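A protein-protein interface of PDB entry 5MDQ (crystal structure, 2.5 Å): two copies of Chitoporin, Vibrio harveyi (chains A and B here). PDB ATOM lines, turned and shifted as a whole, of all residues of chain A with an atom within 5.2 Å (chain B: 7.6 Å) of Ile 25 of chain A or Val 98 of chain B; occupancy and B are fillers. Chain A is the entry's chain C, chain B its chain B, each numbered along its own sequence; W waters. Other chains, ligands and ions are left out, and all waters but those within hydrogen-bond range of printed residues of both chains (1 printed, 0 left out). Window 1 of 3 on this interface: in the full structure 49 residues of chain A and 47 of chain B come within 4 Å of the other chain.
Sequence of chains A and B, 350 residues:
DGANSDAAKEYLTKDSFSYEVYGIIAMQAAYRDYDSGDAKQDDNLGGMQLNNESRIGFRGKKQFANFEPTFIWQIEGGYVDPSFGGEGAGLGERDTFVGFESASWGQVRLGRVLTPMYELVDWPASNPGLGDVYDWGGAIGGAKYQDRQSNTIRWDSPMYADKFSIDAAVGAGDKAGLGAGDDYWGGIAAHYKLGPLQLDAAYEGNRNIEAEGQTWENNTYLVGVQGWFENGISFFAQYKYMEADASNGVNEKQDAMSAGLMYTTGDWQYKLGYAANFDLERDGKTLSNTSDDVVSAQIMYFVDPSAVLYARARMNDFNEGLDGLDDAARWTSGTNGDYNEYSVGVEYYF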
ATOM      1  N   GLY A  23     -17.322  18.964  -7.424  1.00  0.00           N
ATOM      2  CA  GLY A  23     -16.098  19.342  -6.754  1.00  0.00           C
ATOM      3  C   GLY A  23     -16.226  20.059  -5.451  1.00  0.00           C
ATOM      4  O   GLY A  23     -17.269  20.655  -5.116  1.00  0.00           O
ATOM      5  N   ILE A  24     -15.160  19.936  -4.664  1.00  0.00           N
ATOM      6  CA  ILE A  24     -15.019  20.746  -3.455  1.00  0.00           C
ATOM      7  C   ILE A  24     -13.869  21.705  -3.725  1.00  0.00           C
ATOM      8  O   ILE A  24     -12.748  21.276  -4.015  1.00  0.00           O
ATOM      9  CB  ILE A  24     -14.798  19.928  -2.146  1.00  0.00           C
ATOM     10  CG1 ILE A  24     -16.068  19.135  -1.822  1.00  0.00           C
ATOM     11  CG2 ILE A  24     -14.405  20.875  -0.948  1.00  0.00           C
ATOM     12  CD1 ILE A  24     -16.299  17.929  -2.701  1.00  0.00           C
ATOM     13  N   ILE A  25     -14.191  22.992  -3.737  1.00  0.00           N
ATOM     14  CA  ILE A  25     -13.196  24.030  -3.865  1.00  0.00           C
ATOM     15  C   ILE A  25     -12.830  24.498  -2.483  1.00  0.00           C
ATOM     16  O   ILE A  25     -13.712  25.017  -1.765  1.00  0.00           O
ATOM     17  CB  ILE A  25     -13.748  25.207  -4.693  1.00  0.00           C
ATOM     18  CG1 ILE A  25     -14.171  24.748  -6.099  1.00  0.00           C
ATOM     19  CG2 ILE A  25     -12.691  26.259  -4.854  1.00  0.00           C
ATOM     20  CD1 ILE A  25     -13.092  24.011  -6.891  1.00  0.00           C
ATOM     21  N   ALA A  26     -11.545  24.340  -2.138  1.00  0.00           N
ATOM     22  CA  ALA A  26     -11.061  24.532  -0.781  1.00  0.00           C
ATOM     23  C   ALA A  26      -9.675  25.111  -0.751  1.00  0.00           C
ATOM     24  O   ALA A  26      -8.796  24.572  -1.352  1.00  0.00           O
ATOM     25  CB  ALA A  26     -11.070  23.208  -0.037  1.00  0.00           C
ATOM     26  N   MET A  27      -9.540  26.228  -0.073  1.00  0.00           N
ATOM     27  CA  MET A  27      -8.298  27.073  -0.016  1.00  0.00           C
ATOM     28  C   MET A  27      -8.152  27.649   1.404  1.00  0.00           C
ATOM     29  O   MET A  27      -9.079  28.252   1.930  1.00  0.00           O
ATOM     30  CB  MET A  27      -8.333  28.289  -0.981  1.00  0.00           C
ATOM     31  CG  MET A  27      -7.045  29.116  -0.935  1.00  0.00           C
ATOM     32  SD  MET A  27      -5.482  28.210  -1.342  1.00  0.00           S
ATOM     33  CE  MET A  27      -5.589  28.356  -3.126  1.00  0.00           C
ATOM     34  N   SER A  54      -8.542  21.914  -3.154  1.00  0.00           N
ATOM     35  CA  SER A  54      -9.590  21.749  -4.139  1.00  0.00           C
ATOM     36  C   SER A  54      -9.430  20.360  -4.834  1.00  0.00           C
ATOM     37  O   SER A  54      -8.298  19.866  -5.048  1.00  0.00           O
ATOM     38  CB  SER A  54      -9.563  22.930  -5.172  1.00  0.00           C
ATOM     39  OG  SER A  54      -9.846  24.201  -4.560  1.00  0.00           O
ATOM     40  N   ARG A  55     -10.561  19.724  -5.127  1.00  0.00           N
ATOM     41  CA  ARG A  55     -10.611  18.510  -5.904  1.00  0.00           C
ATOM     42  C   ARG A  55     -11.859  18.390  -6.762  1.00  0.00           C
ATOM     43  O   ARG A  55     -12.947  18.960  -6.504  1.00  0.00           O
ATOM     44  CB  ARG A  55     -10.427  17.310  -5.045  1.00  0.00           C
ATOM     45  CG  ARG A  55     -11.554  17.014  -3.985  1.00  0.00           C
ATOM     46  CD  ARG A  55     -11.181  17.650  -2.714  1.00  0.00           C
ATOM     47  NE  ARG A  55     -12.040  17.344  -1.582  1.00  0.00           N
ATOM     48  CZ  ARG A  55     -12.214  18.087  -0.482  1.00  0.00           C
ATOM     49  NH1 ARG A  55     -11.538  19.177  -0.355  1.00  0.00           N
ATOM     50  NH2 ARG A  55     -12.960  17.684   0.506  1.00  0.00           N
ATOM     51  N   VAL A 346     -11.749  29.162   2.726  1.00  0.00           N
ATOM     52  CA  VAL A 346     -13.061  29.089   2.084  1.00  0.00           C
ATOM     53  C   VAL A 346     -13.258  27.693   1.531  1.00  0.00           C
ATOM     54  O   VAL A 346     -12.276  27.061   1.089  1.00  0.00           O
ATOM     55  CB  VAL A 346     -13.174  30.144   0.953  1.00  0.00           C
ATOM     56  CG1 VAL A 346     -12.023  30.034  -0.056  1.00  0.00           C
ATOM     57  CG2 VAL A 346     -14.482  30.010   0.206  1.00  0.00           C
ATOM     58  N   GLU A 347     -14.509  27.202   1.601  1.00  0.00           N
ATOM     59  CA  GLU A 347     -14.902  25.897   1.058  1.00  0.00           C
ATOM     60  C   GLU A 347     -16.248  26.055   0.379  1.00  0.00           C
ATOM     61  O   GLU A 347     -17.090  26.742   0.906  1.00  0.00           O
ATOM     62  CB  GLU A 347     -14.945  24.778   2.105  1.00  0.00           C
ATOM     63  CG  GLU A 347     -13.648  24.639   2.933  1.00  0.00           C
ATOM     64  CD  GLU A 347     -13.169  23.228   3.117  1.00  0.00           C
ATOM     65  OE1 GLU A 347     -13.849  22.320   2.657  1.00  0.00           O
ATOM     66  OE2 GLU A 347     -12.088  22.997   3.704  1.00  0.00           O
ATOM     67  N   TYR A 348     -16.351  25.485  -0.833  1.00  0.00           N
ATOM     68  CA  TYR A 348     -17.512  25.590  -1.716  1.00  0.00           C
ATOM     69  C   TYR A 348     -17.747  24.202  -2.390  1.00  0.00           C
ATOM     70  O   TYR A 348     -16.792  23.630  -2.928  1.00  0.00           O
ATOM     71  CB  TYR A 348     -17.249  26.601  -2.795  1.00  0.00           C
ATOM     72  CG  TYR A 348     -18.242  26.667  -3.970  1.00  0.00           C
ATOM     73  CD1 TYR A 348     -19.554  27.000  -3.792  1.00  0.00           C
ATOM     74  CD2 TYR A 348     -17.821  26.415  -5.309  1.00  0.00           C
ATOM     75  CE1 TYR A 348     -20.453  27.065  -4.853  1.00  0.00           C
ATOM     76  CE2 TYR A 348     -18.724  26.497  -6.374  1.00  0.00           C
ATOM     77  CZ  TYR A 348     -20.033  26.810  -6.106  1.00  0.00           C
ATOM     78  OH  TYR A 348     -20.904  26.836  -7.115  1.00  0.00           O
ATOM     79  N   TYR A 349     -19.001  23.753  -2.447  1.00  0.00           N
ATOM     80  CA  TYR A 349     -19.337  22.497  -3.032  1.00  0.00           C
ATOM     81  C   TYR A 349     -20.245  22.724  -4.233  1.00  0.00           C
ATOM     82  O   TYR A 349     -21.348  23.303  -4.088  1.00  0.00           O
ATOM     83  CB  TYR A 349     -20.096  21.717  -1.964  1.00  0.00           C
ATOM     84  CG  TYR A 349     -20.525  20.334  -2.302  1.00  0.00           C
ATOM     85  CD1 TYR A 349     -19.772  19.522  -3.187  1.00  0.00           C
ATOM     86  CD2 TYR A 349     -21.725  19.778  -1.688  1.00  0.00           C
ATOM     87  CE1 TYR A 349     -20.167  18.242  -3.472  1.00  0.00           C
ATOM     88  CE2 TYR A 349     -22.116  18.475  -1.952  1.00  0.00           C
ATOM     89  CZ  TYR A 349     -21.343  17.696  -2.849  1.00  0.00           C
ATOM     90  OH  TYR A 349     -21.690  16.415  -3.177  1.00  0.00           O
ATOM     91  N   PHE A 350     -19.847  22.202  -5.391  1.00  0.00           N
ATOM     92  CA  PHE A 350     -20.752  22.126  -6.544  1.00  0.00           C
ATOM     93  C   PHE A 350     -20.896  20.705  -7.023  1.00  0.00           C
ATOM     94  O   PHE A 350     -21.892  20.510  -7.702  1.00  0.00           O
ATOM     95  CB  PHE A 350     -20.292  22.955  -7.677  1.00  0.00           C
ATOM     96  CG  PHE A 350     -19.117  22.388  -8.349  1.00  0.00           C
ATOM     97  CD1 PHE A 350     -17.818  22.709  -7.888  1.00  0.00           C
ATOM     98  CD2 PHE A 350     -19.269  21.533  -9.452  1.00  0.00           C
ATOM     99  CE1 PHE A 350     -16.710  22.218  -8.536  1.00  0.00           C
ATOM    100  CE2 PHE A 350     -18.141  21.035 -10.104  1.00  0.00           C
ATOM    101  CZ  PHE A 350     -16.872  21.362  -9.632  1.00  0.00           C
ATOM    102  OXT PHE A 350     -20.069  19.793  -6.799  1.00  0.00           O
ATOM    103  N   ALA B   8     -17.716  19.647   3.778  1.00  0.00           N
ATOM    104  CA  ALA B   8     -18.414  20.384   2.728  1.00  0.00           C
ATOM    105  C   ALA B   8     -19.465  19.538   2.019  1.00  0.00           C
ATOM    106  O   ALA B   8     -20.643  19.906   1.971  1.00  0.00           O
ATOM    107  CB  ALA B   8     -17.429  20.936   1.721  1.00  0.00           C
ATOM    108  N   LEU B  12     -22.905  21.136   3.242  1.00  0.00           N
ATOM    109  CA  LEU B  12     -23.284  22.243   2.316  1.00  0.00           C
ATOM    110  C   LEU B  12     -24.267  21.840   1.219  1.00  0.00           C
ATOM    111  O   LEU B  12     -24.281  20.696   0.819  1.00  0.00           O
ATOM    112  CB  LEU B  12     -22.035  22.855   1.723  1.00  0.00           C
ATOM    113  CG  LEU B  12     -20.995  23.405   2.708  1.00  0.00           C
ATOM    114  CD1 LEU B  12     -19.747  23.891   1.979  1.00  0.00           C
ATOM    115  CD2 LEU B  12     -21.580  24.550   3.470  1.00  0.00           C
ATOM    116  N   PHE B  58     -11.262  23.158 -15.430  1.00  0.00           N
ATOM    117  CA  PHE B  58     -12.561  23.386 -14.795  1.00  0.00           C
ATOM    118  C   PHE B  58     -12.600  24.802 -14.150  1.00  0.00           C
ATOM    119  O   PHE B  58     -11.607  25.231 -13.527  1.00  0.00           O
ATOM    120  CB  PHE B  58     -12.784  22.382 -13.690  1.00  0.00           C
ATOM    121  CG  PHE B  58     -12.793  20.952 -14.156  1.00  0.00           C
ATOM    122  CD1 PHE B  58     -11.578  20.251 -14.258  1.00  0.00           C
ATOM    123  CD2 PHE B  58     -13.997  20.321 -14.477  1.00  0.00           C
ATOM    124  CE1 PHE B  58     -11.543  19.000 -14.731  1.00  0.00           C
ATOM    125  CE2 PHE B  58     -13.971  19.019 -14.941  1.00  0.00           C
ATOM    126  CZ  PHE B  58     -12.720  18.371 -15.090  1.00  0.00           C
ATOM    127  N   ARG B  59     -13.741  25.484 -14.265  1.00  0.00           N
ATOM    128  CA  ARG B  59     -13.872  26.845 -13.685  1.00  0.00           C
ATOM    129  C   ARG B  59     -15.316  27.275 -13.449  1.00  0.00           C
ATOM    130  O   ARG B  59     -16.262  26.674 -14.019  1.00  0.00           O
ATOM    131  CB  ARG B  59     -13.143  27.887 -14.562  1.00  0.00           C
ATOM    132  CG  ARG B  59     -13.748  28.008 -15.940  1.00  0.00           C
ATOM    133  CD  ARG B  59     -12.867  28.851 -16.862  1.00  0.00           C
ATOM    134  NE  ARG B  59     -13.422  28.802 -18.192  1.00  0.00           N
ATOM    135  CZ  ARG B  59     -12.761  29.015 -19.321  1.00  0.00           C
ATOM    136  NH1 ARG B  59     -11.460  29.361 -19.335  1.00  0.00           N
ATOM    137  NH2 ARG B  59     -13.397  28.884 -20.477  1.00  0.00           N
ATOM    138  N   GLY B  60     -15.456  28.283 -12.582  1.00  0.00           N
ATOM    139  CA  GLY B  60     -16.736  28.868 -12.365  1.00  0.00           C
ATOM    140  C   GLY B  60     -16.767  30.091 -11.503  1.00  0.00           C
ATOM    141  O   GLY B  60     -15.728  30.493 -10.933  1.00  0.00           O
ATOM    142  N   PHE B  71     -17.343  35.136  -6.126  1.00  0.00           N
ATOM    143  CA  PHE B  71     -16.333  34.138  -5.921  1.00  0.00           C
ATOM    144  C   PHE B  71     -16.004  33.583  -7.303  1.00  0.00           C
ATOM    145  O   PHE B  71     -16.931  33.391  -8.098  1.00  0.00           O
ATOM    146  CB  PHE B  71     -16.943  32.981  -5.061  1.00  0.00           C
ATOM    147  CG  PHE B  71     -15.964  31.862  -4.732  1.00  0.00           C
ATOM    148  CD1 PHE B  71     -14.806  32.112  -4.000  1.00  0.00           C
ATOM    149  CD2 PHE B  71     -16.232  30.555  -5.120  1.00  0.00           C
ATOM    150  CE1 PHE B  71     -13.875  31.114  -3.699  1.00  0.00           C
ATOM    151  CE2 PHE B  71     -15.347  29.518  -4.778  1.00  0.00           C
ATOM    152  CZ  PHE B  71     -14.152  29.801  -4.071  1.00  0.00           C
ATOM    153  N   ILE B  72     -14.731  33.308  -7.574  1.00  0.00           N
ATOM    154  CA  ILE B  72     -14.290  32.688  -8.800  1.00  0.00           C
ATOM    155  C   ILE B  72     -13.289  31.603  -8.438  1.00  0.00           C
ATOM    156  O   ILE B  72     -12.586  31.709  -7.410  1.00  0.00           O
ATOM    157  CB  ILE B  72     -13.580  33.666  -9.707  1.00  0.00           C
ATOM    158  CG1 ILE B  72     -12.343  34.255  -9.011  1.00  0.00           C
ATOM    159  CG2 ILE B  72     -14.535  34.763 -10.130  1.00  0.00           C
ATOM    160  CD1 ILE B  72     -11.446  35.018  -9.916  1.00  0.00           C
ATOM    161  N   TRP B  73     -13.211  30.570  -9.272  1.00  0.00           N
ATOM    162  CA  TRP B  73     -12.274  29.454  -9.062  1.00  0.00           C
ATOM    163  C   TRP B  73     -11.942  28.840 -10.421  1.00  0.00           C
ATOM    164  O   TRP B  73     -12.660  28.974 -11.423  1.00  0.00           O
ATOM    165  CB  TRP B  73     -12.826  28.367  -8.097  1.00  0.00           C
ATOM    166  CG  TRP B  73     -14.068  27.759  -8.607  1.00  0.00           C
ATOM    167  CD1 TRP B  73     -15.376  28.219  -8.428  1.00  0.00           C
ATOM    168  CD2 TRP B  73     -14.165  26.606  -9.393  1.00  0.00           C
ATOM    169  NE1 TRP B  73     -16.257  27.442  -9.111  1.00  0.00           N
ATOM    170  CE2 TRP B  73     -15.546  26.431  -9.720  1.00  0.00           C
ATOM    171  CE3 TRP B  73     -13.232  25.704  -9.874  1.00  0.00           C
ATOM    172  CZ2 TRP B  73     -15.996  25.377 -10.519  1.00  0.00           C
ATOM    173  CZ3 TRP B  73     -13.676  24.653 -10.674  1.00  0.00           C
ATOM    174  CH2 TRP B  73     -15.063  24.474 -10.944  1.00  0.00           C
ATOM    175  N   GLN B  74     -10.804  28.179 -10.438  1.00  0.00           N
ATOM    176  CA  GLN B  74     -10.387  27.456 -11.599  1.00  0.00           C
ATOM    177  C   GLN B  74      -9.363  26.386 -11.214  1.00  0.00           C
ATOM    178  O   GLN B  74      -8.537  26.612 -10.321  1.00  0.00           O
ATOM    179  CB  GLN B  74      -9.763  28.438 -12.653  1.00  0.00           C
ATOM    180  CG  GLN B  74      -8.996  27.769 -13.801  1.00  0.00           C
ATOM    181  CD  GLN B  74      -8.507  28.797 -14.758  1.00  0.00           C
ATOM    182  OE1 GLN B  74      -9.303  29.533 -15.255  1.00  0.00           O
ATOM    183  NE2 GLN B  74      -7.183  28.892 -14.984  1.00  0.00           N
ATOM    184  N   ILE B  75      -9.391  25.296 -11.974  1.00  0.00           N
ATOM    185  CA  ILE B  75      -8.441  24.199 -11.854  1.00  0.00           C
ATOM    186  C   ILE B  75      -8.115  23.663 -13.237  1.00  0.00           C
ATOM    187  O   ILE B  75      -9.009  23.152 -13.967  1.00  0.00           O
ATOM    188  CB  ILE B  75      -9.060  22.998 -11.114  1.00  0.00           C
ATOM    189  CG1 ILE B  75      -9.596  23.406  -9.725  1.00  0.00           C
ATOM    190  CG2 ILE B  75      -8.011  21.896 -11.020  1.00  0.00           C
ATOM    191  CD1 ILE B  75     -10.335  22.365  -8.934  1.00  0.00           C
ATOM    192  N   THR B  96      -4.411  27.591 -11.339  1.00  0.00           N
ATOM    193  CA  THR B  96      -5.314  26.875 -10.479  1.00  0.00           C
ATOM    194  C   THR B  96      -5.465  27.718  -9.190  1.00  0.00           C
ATOM    195  O   THR B  96      -4.477  27.971  -8.503  1.00  0.00           O
ATOM    196  CB  THR B  96      -4.722  25.502 -10.267  1.00  0.00           C
ATOM    197  OG1 THR B  96      -4.869  24.750 -11.497  1.00  0.00           O
ATOM    198  CG2 THR B  96      -5.412  24.808  -9.100  1.00  0.00           C
ATOM    199  N   PHE B  97      -6.674  28.233  -8.943  1.00  0.00           N
ATOM    200  CA  PHE B  97      -6.844  29.241  -7.929  1.00  0.00           C
ATOM    201  C   PHE B  97      -8.280  29.409  -7.494  1.00  0.00           C
ATOM    202  O   PHE B  97      -9.222  28.916  -8.104  1.00  0.00           O
ATOM    203  CB  PHE B  97      -6.315  30.601  -8.451  1.00  0.00           C
ATOM    204  CG  PHE B  97      -6.986  31.076  -9.730  1.00  0.00           C
ATOM    205  CD1 PHE B  97      -8.260  31.635  -9.724  1.00  0.00           C
ATOM    206  CD2 PHE B  97      -6.350  30.903 -10.972  1.00  0.00           C
ATOM    207  CE1 PHE B  97      -8.882  32.041 -10.897  1.00  0.00           C
ATOM    208  CE2 PHE B  97      -6.987  31.329 -12.133  1.00  0.00           C
ATOM    209  CZ  PHE B  97      -8.258  31.921 -12.087  1.00  0.00           C
ATOM    210  N   VAL B  98      -8.419  30.173  -6.415  1.00  0.00           N
ATOM    211  CA  VAL B  98      -9.704  30.785  -6.039  1.00  0.00           C
ATOM    212  C   VAL B  98      -9.538  32.291  -6.024  1.00  0.00           C
ATOM    213  O   VAL B  98      -8.420  32.784  -5.915  1.00  0.00           O
ATOM    214  CB  VAL B  98     -10.196  30.326  -4.621  1.00  0.00           C
ATOM    215  CG1 VAL B  98     -10.160  28.796  -4.480  1.00  0.00           C
ATOM    216  CG2 VAL B  98      -9.329  30.899  -3.540  1.00  0.00           C
ATOM    217  N   GLY B  99     -10.642  33.014  -6.031  1.00  0.00           N
ATOM    218  CA  GLY B  99     -10.563  34.435  -5.793  1.00  0.00           C
ATOM    219  C   GLY B  99     -11.889  35.134  -5.728  1.00  0.00           C
ATOM    220  O   GLY B  99     -12.926  34.506  -5.596  1.00  0.00           O
ATOM    221  N   PHE B 100     -11.845  36.452  -5.898  1.00  0.00           N
ATOM    222  CA  PHE B 100     -13.020  37.307  -5.700  1.00  0.00           C
ATOM    223  C   PHE B 100     -12.960  38.482  -6.624  1.00  0.00           C
ATOM    224  O   PHE B 100     -11.849  38.910  -7.029  1.00  0.00           O
ATOM    225  CB  PHE B 100     -13.020  37.872  -4.283  1.00  0.00           C
ATOM    226  CG  PHE B 100     -13.423  36.882  -3.240  1.00  0.00           C
ATOM    227  CD1 PHE B 100     -14.762  36.503  -3.134  1.00  0.00           C
ATOM    228  CD2 PHE B 100     -12.469  36.278  -2.436  1.00  0.00           C
ATOM    229  CE1 PHE B 100     -15.142  35.568  -2.238  1.00  0.00           C
ATOM    230  CE2 PHE B 100     -12.831  35.297  -1.564  1.00  0.00           C
ATOM    231  CZ  PHE B 100     -14.178  34.958  -1.445  1.00  0.00           C
ATOM    232  N   VAL B 108      -8.881  39.650  -7.266  1.00  0.00           N
ATOM    233  CA  VAL B 108      -7.814  39.052  -6.483  1.00  0.00           C
ATOM    234  C   VAL B 108      -7.959  37.490  -6.580  1.00  0.00           C
ATOM    235  O   VAL B 108      -9.057  36.938  -6.442  1.00  0.00           O
ATOM    236  CB  VAL B 108      -7.750  39.531  -4.980  1.00  0.00           C
ATOM    237  CG1 VAL B 108      -9.051  39.324  -4.220  1.00  0.00           C
ATOM    238  CG2 VAL B 108      -6.630  38.886  -4.156  1.00  0.00           C
ATOM    239  N   ARG B 109      -6.828  36.843  -6.836  1.00  0.00           N
ATOM    240  CA  ARG B 109      -6.704  35.453  -6.993  1.00  0.00           C
ATOM    241  C   ARG B 109      -5.639  35.012  -6.025  1.00  0.00           C
ATOM    242  O   ARG B 109      -4.648  35.716  -5.828  1.00  0.00           O
ATOM    243  CB  ARG B 109      -6.292  35.092  -8.401  1.00  0.00           C
ATOM    244  CG  ARG B 109      -7.417  35.259  -9.422  1.00  0.00           C
ATOM    245  CD  ARG B 109      -6.988  34.843 -10.830  1.00  0.00           C
ATOM    246  NE  ARG B 109      -6.106  35.817 -11.400  1.00  0.00           N
ATOM    247  CZ  ARG B 109      -5.219  35.615 -12.386  1.00  0.00           C
ATOM    248  NH1 ARG B 109      -5.129  34.424 -12.964  1.00  0.00           N
ATOM    249  NH2 ARG B 109      -4.442  36.625 -12.795  1.00  0.00           N
ATOM    250  N   LEU B 110      -5.891  33.848  -5.419  1.00  0.00           N
ATOM    251  CA  LEU B 110      -4.978  33.206  -4.542  1.00  0.00           C
ATOM    252  C   LEU B 110      -4.785  31.801  -5.049  1.00  0.00           C
ATOM    253  O   LEU B 110      -5.758  31.040  -5.289  1.00  0.00           O
ATOM    254  CB  LEU B 110      -5.525  33.137  -3.124  1.00  0.00           C
ATOM    255  CG  LEU B 110      -5.754  34.426  -2.335  1.00  0.00           C
ATOM    256  CD1 LEU B 110      -7.200  34.861  -2.540  1.00  0.00           C
ATOM    257  CD2 LEU B 110      -5.575  34.280  -0.813  1.00  0.00           C
ATOM    258  N   GLY B 111      -3.505  31.427  -5.166  1.00  0.00           N
ATOM    259  CA  GLY B 111      -3.118  30.104  -5.632  1.00  0.00           C
ATOM    260  C   GLY B 111      -1.918  30.079  -6.562  1.00  0.00           C
ATOM    261  O   GLY B 111      -0.772  30.458  -6.182  1.00  0.00           O
ATOM    262  N   ARG B 112      -2.143  29.518  -7.739  1.00  0.00           N
ATOM    263  CA  ARG B 112      -1.081  29.251  -8.681  1.00  0.00           C
ATOM    264  C   ARG B 112      -1.425  30.014  -9.947  1.00  0.00           C
ATOM    265  O   ARG B 112      -2.467  29.738 -10.599  1.00  0.00           O
ATOM    266  CB  ARG B 112      -0.992  27.812  -8.973  1.00  0.00           C
ATOM    267  CG  ARG B 112      -0.064  27.427 -10.123  1.00  0.00           C
ATOM    268  CD  ARG B 112       0.060  25.887 -10.186  1.00  0.00           C
ATOM    269  NE  ARG B 112       1.118  25.468 -11.094  1.00  0.00           N
ATOM    270  CZ  ARG B 112       2.424  25.578 -10.847  1.00  0.00           C
ATOM    271  NH1 ARG B 112       2.886  26.099  -9.752  1.00  0.00           N
ATOM    272  NH2 ARG B 112       3.293  25.256 -11.762  1.00  0.00           N
ATOM    273  N   VAL B 113      -0.615  31.032 -10.242  1.00  0.00           N
ATOM    274  CA  VAL B 113      -0.904  31.964 -11.352  1.00  0.00           C
ATOM    275  C   VAL B 113       0.394  32.428 -11.901  1.00  0.00           C
ATOM    276  O   VAL B 113       1.481  32.134 -11.370  1.00  0.00           O
ATOM    277  CB  VAL B 113      -1.737  33.206 -10.910  1.00  0.00           C
ATOM    278  CG1 VAL B 113      -3.135  32.815 -10.388  1.00  0.00           C
ATOM    279  CG2 VAL B 113      -0.971  33.985  -9.867  1.00  0.00           C
ATOM    280  N   THR B 152       0.684  32.192  -4.193  1.00  0.00           N
ATOM    281  CA  THR B 152       0.720  33.499  -4.765  1.00  0.00           C
ATOM    282  C   THR B 152      -0.600  34.173  -4.536  1.00  0.00           C
ATOM    283  O   THR B 152      -1.636  33.565  -4.753  1.00  0.00           O
ATOM    284  CB  THR B 152       0.992  33.369  -6.290  1.00  0.00           C
ATOM    285  OG1 THR B 152       2.321  32.843  -6.457  1.00  0.00           O
ATOM    286  CG2 THR B 152       0.893  34.721  -7.012  1.00  0.00           C
ATOM    287  N   ARG B 154      -2.414  37.604  -6.075  1.00  0.00           N
ATOM    288  CA  ARG B 154      -2.300  38.482  -7.171  1.00  0.00           C
ATOM    289  C   ARG B 154      -3.577  39.292  -7.395  1.00  0.00           C
ATOM    290  O   ARG B 154      -4.679  38.729  -7.457  1.00  0.00           O
ATOM    291  CB  ARG B 154      -2.009  37.686  -8.432  1.00  0.00           C
ATOM    292  CG  ARG B 154      -2.195  38.519  -9.687  1.00  0.00           C
ATOM    293  CD  ARG B 154      -1.495  37.984 -10.922  1.00  0.00           C
ATOM    294  NE  ARG B 154      -2.012  38.686 -12.093  1.00  0.00           N
ATOM    295  CZ  ARG B 154      -1.514  38.632 -13.315  1.00  0.00           C
ATOM    296  NH1 ARG B 154      -0.447  37.923 -13.609  1.00  0.00           N
ATOM    297  NH2 ARG B 154      -2.088  39.340 -14.269  1.00  0.00           N
HETATM  298  O   HOH W   1      -8.369  25.986  -6.871  1.00  0.00           O
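Water W1 bridges the side-chain hydroxyl (OG) of Ser 54 of chain A (3.3 Å) and the backbone carbonyl oxygen (O) of Phe 97 of chain B (3.3 Å).
N of Ala 26 of chain A is in hydrogen-bond range of OG of Ser 54 of chain A (3.0 Å).
The backbone NH of Val 346 of chain A lies within hydrogen-bond range of the backbone carbonyl oxygen of Met 27 of chain A (2.9 Å).
N of Trp 73 of chain B lies within hydrogen-bond range of O of Gly 60 of chain B, 3.0 Å away.
The backbone NH (N) of Ile 25 of chain A sits at hydrogen-bond distance from the backbone carbonyl oxygen (O) of Tyr 348 of chain A (2.8 Å).
The backbone NH of Gly 111 of chain B is in hydrogen-bond range of the backbone carbonyl oxygen of Thr 152 of chain B (2.9 Å).
The backbone carbonyl oxygen (O) of Val 98 of chain B sits at hydrogen-bond distance from the backbone NH (N) of Leu 110 of chain B (2.8 Å).
Of the 23 printed residues of chain B, 8 touch a printed residue of chain A.
Hydrophobic or aromatic side chains of chain B that line the printed part of chain A: Ala 8, Phe 71, Trp 73, Ile 75 and Val 98.
Among the printed residues, no Asp or Glu carboxylate lies within 4 Å of a Lys or Arg side-chain nitrogen of the other chain.
No position is printed for both chains.
Of the 13 pairs that touch across the chains among the printed residues, none has its exchanged pair printed and touching as well.
Ile 25 of chain A touches Trp 73 of chain B.
Ile 25 of chain A touches Ile 75 of chain B.
CG1 of Val 98 of chain B touches CG2 of Ile 25 of chain A, at 3.6 Å.
Met 27 of chain A touches Val 98 of chain B (CB to CG2, 3.8 Å).
O of Leu 110 of chain B touches CE of Met 27 of chain A, 3.5 Å away.
CE of Met 27 of chain A touches CA of Gly 111 of chain B (3.9 Å).
Glu 347 of chain A touches Ala 8 of chain B.
CE2 of Tyr 348 of chain A touches NE1 of Trp 73 of chain B, 3.8 Å away.
O of Leu 12 of chain B touches CD2 of Tyr 349 of chain A, 3.7 Å away.
Trp 73 of chain B touches Phe 350 of chain A.
Of chain B, only Phe 71 (3.9 Å), Trp 73 (3.4 Å), Ile 75 (3.8 Å) and Val 98 (3.6 Å) come within 4 Å of Ile 25 of chain A.
Printed residues of chain B within 4 Å of Tyr 348 of chain A: Trp 73.
Of the printed residues of chain A, Leu 12 of chain B touches Tyr 349.
Of the printed residues of chain A, Trp 73 of chain B touches Ile 25 (3.4 Å), Tyr 348 (3.8 Å) and Phe 350 (3.7 Å).
Of the printed residues of chain A, Ile 75 of chain B touches Ile 25 and Ser 54.
Val 98 of chain B touches just these residues of chain A: Ile 25 (3.6 Å) and Met 27 (3.8 Å).
Printed residues of chain A within 4 Å of Leu 110 of chain B: Met 27.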
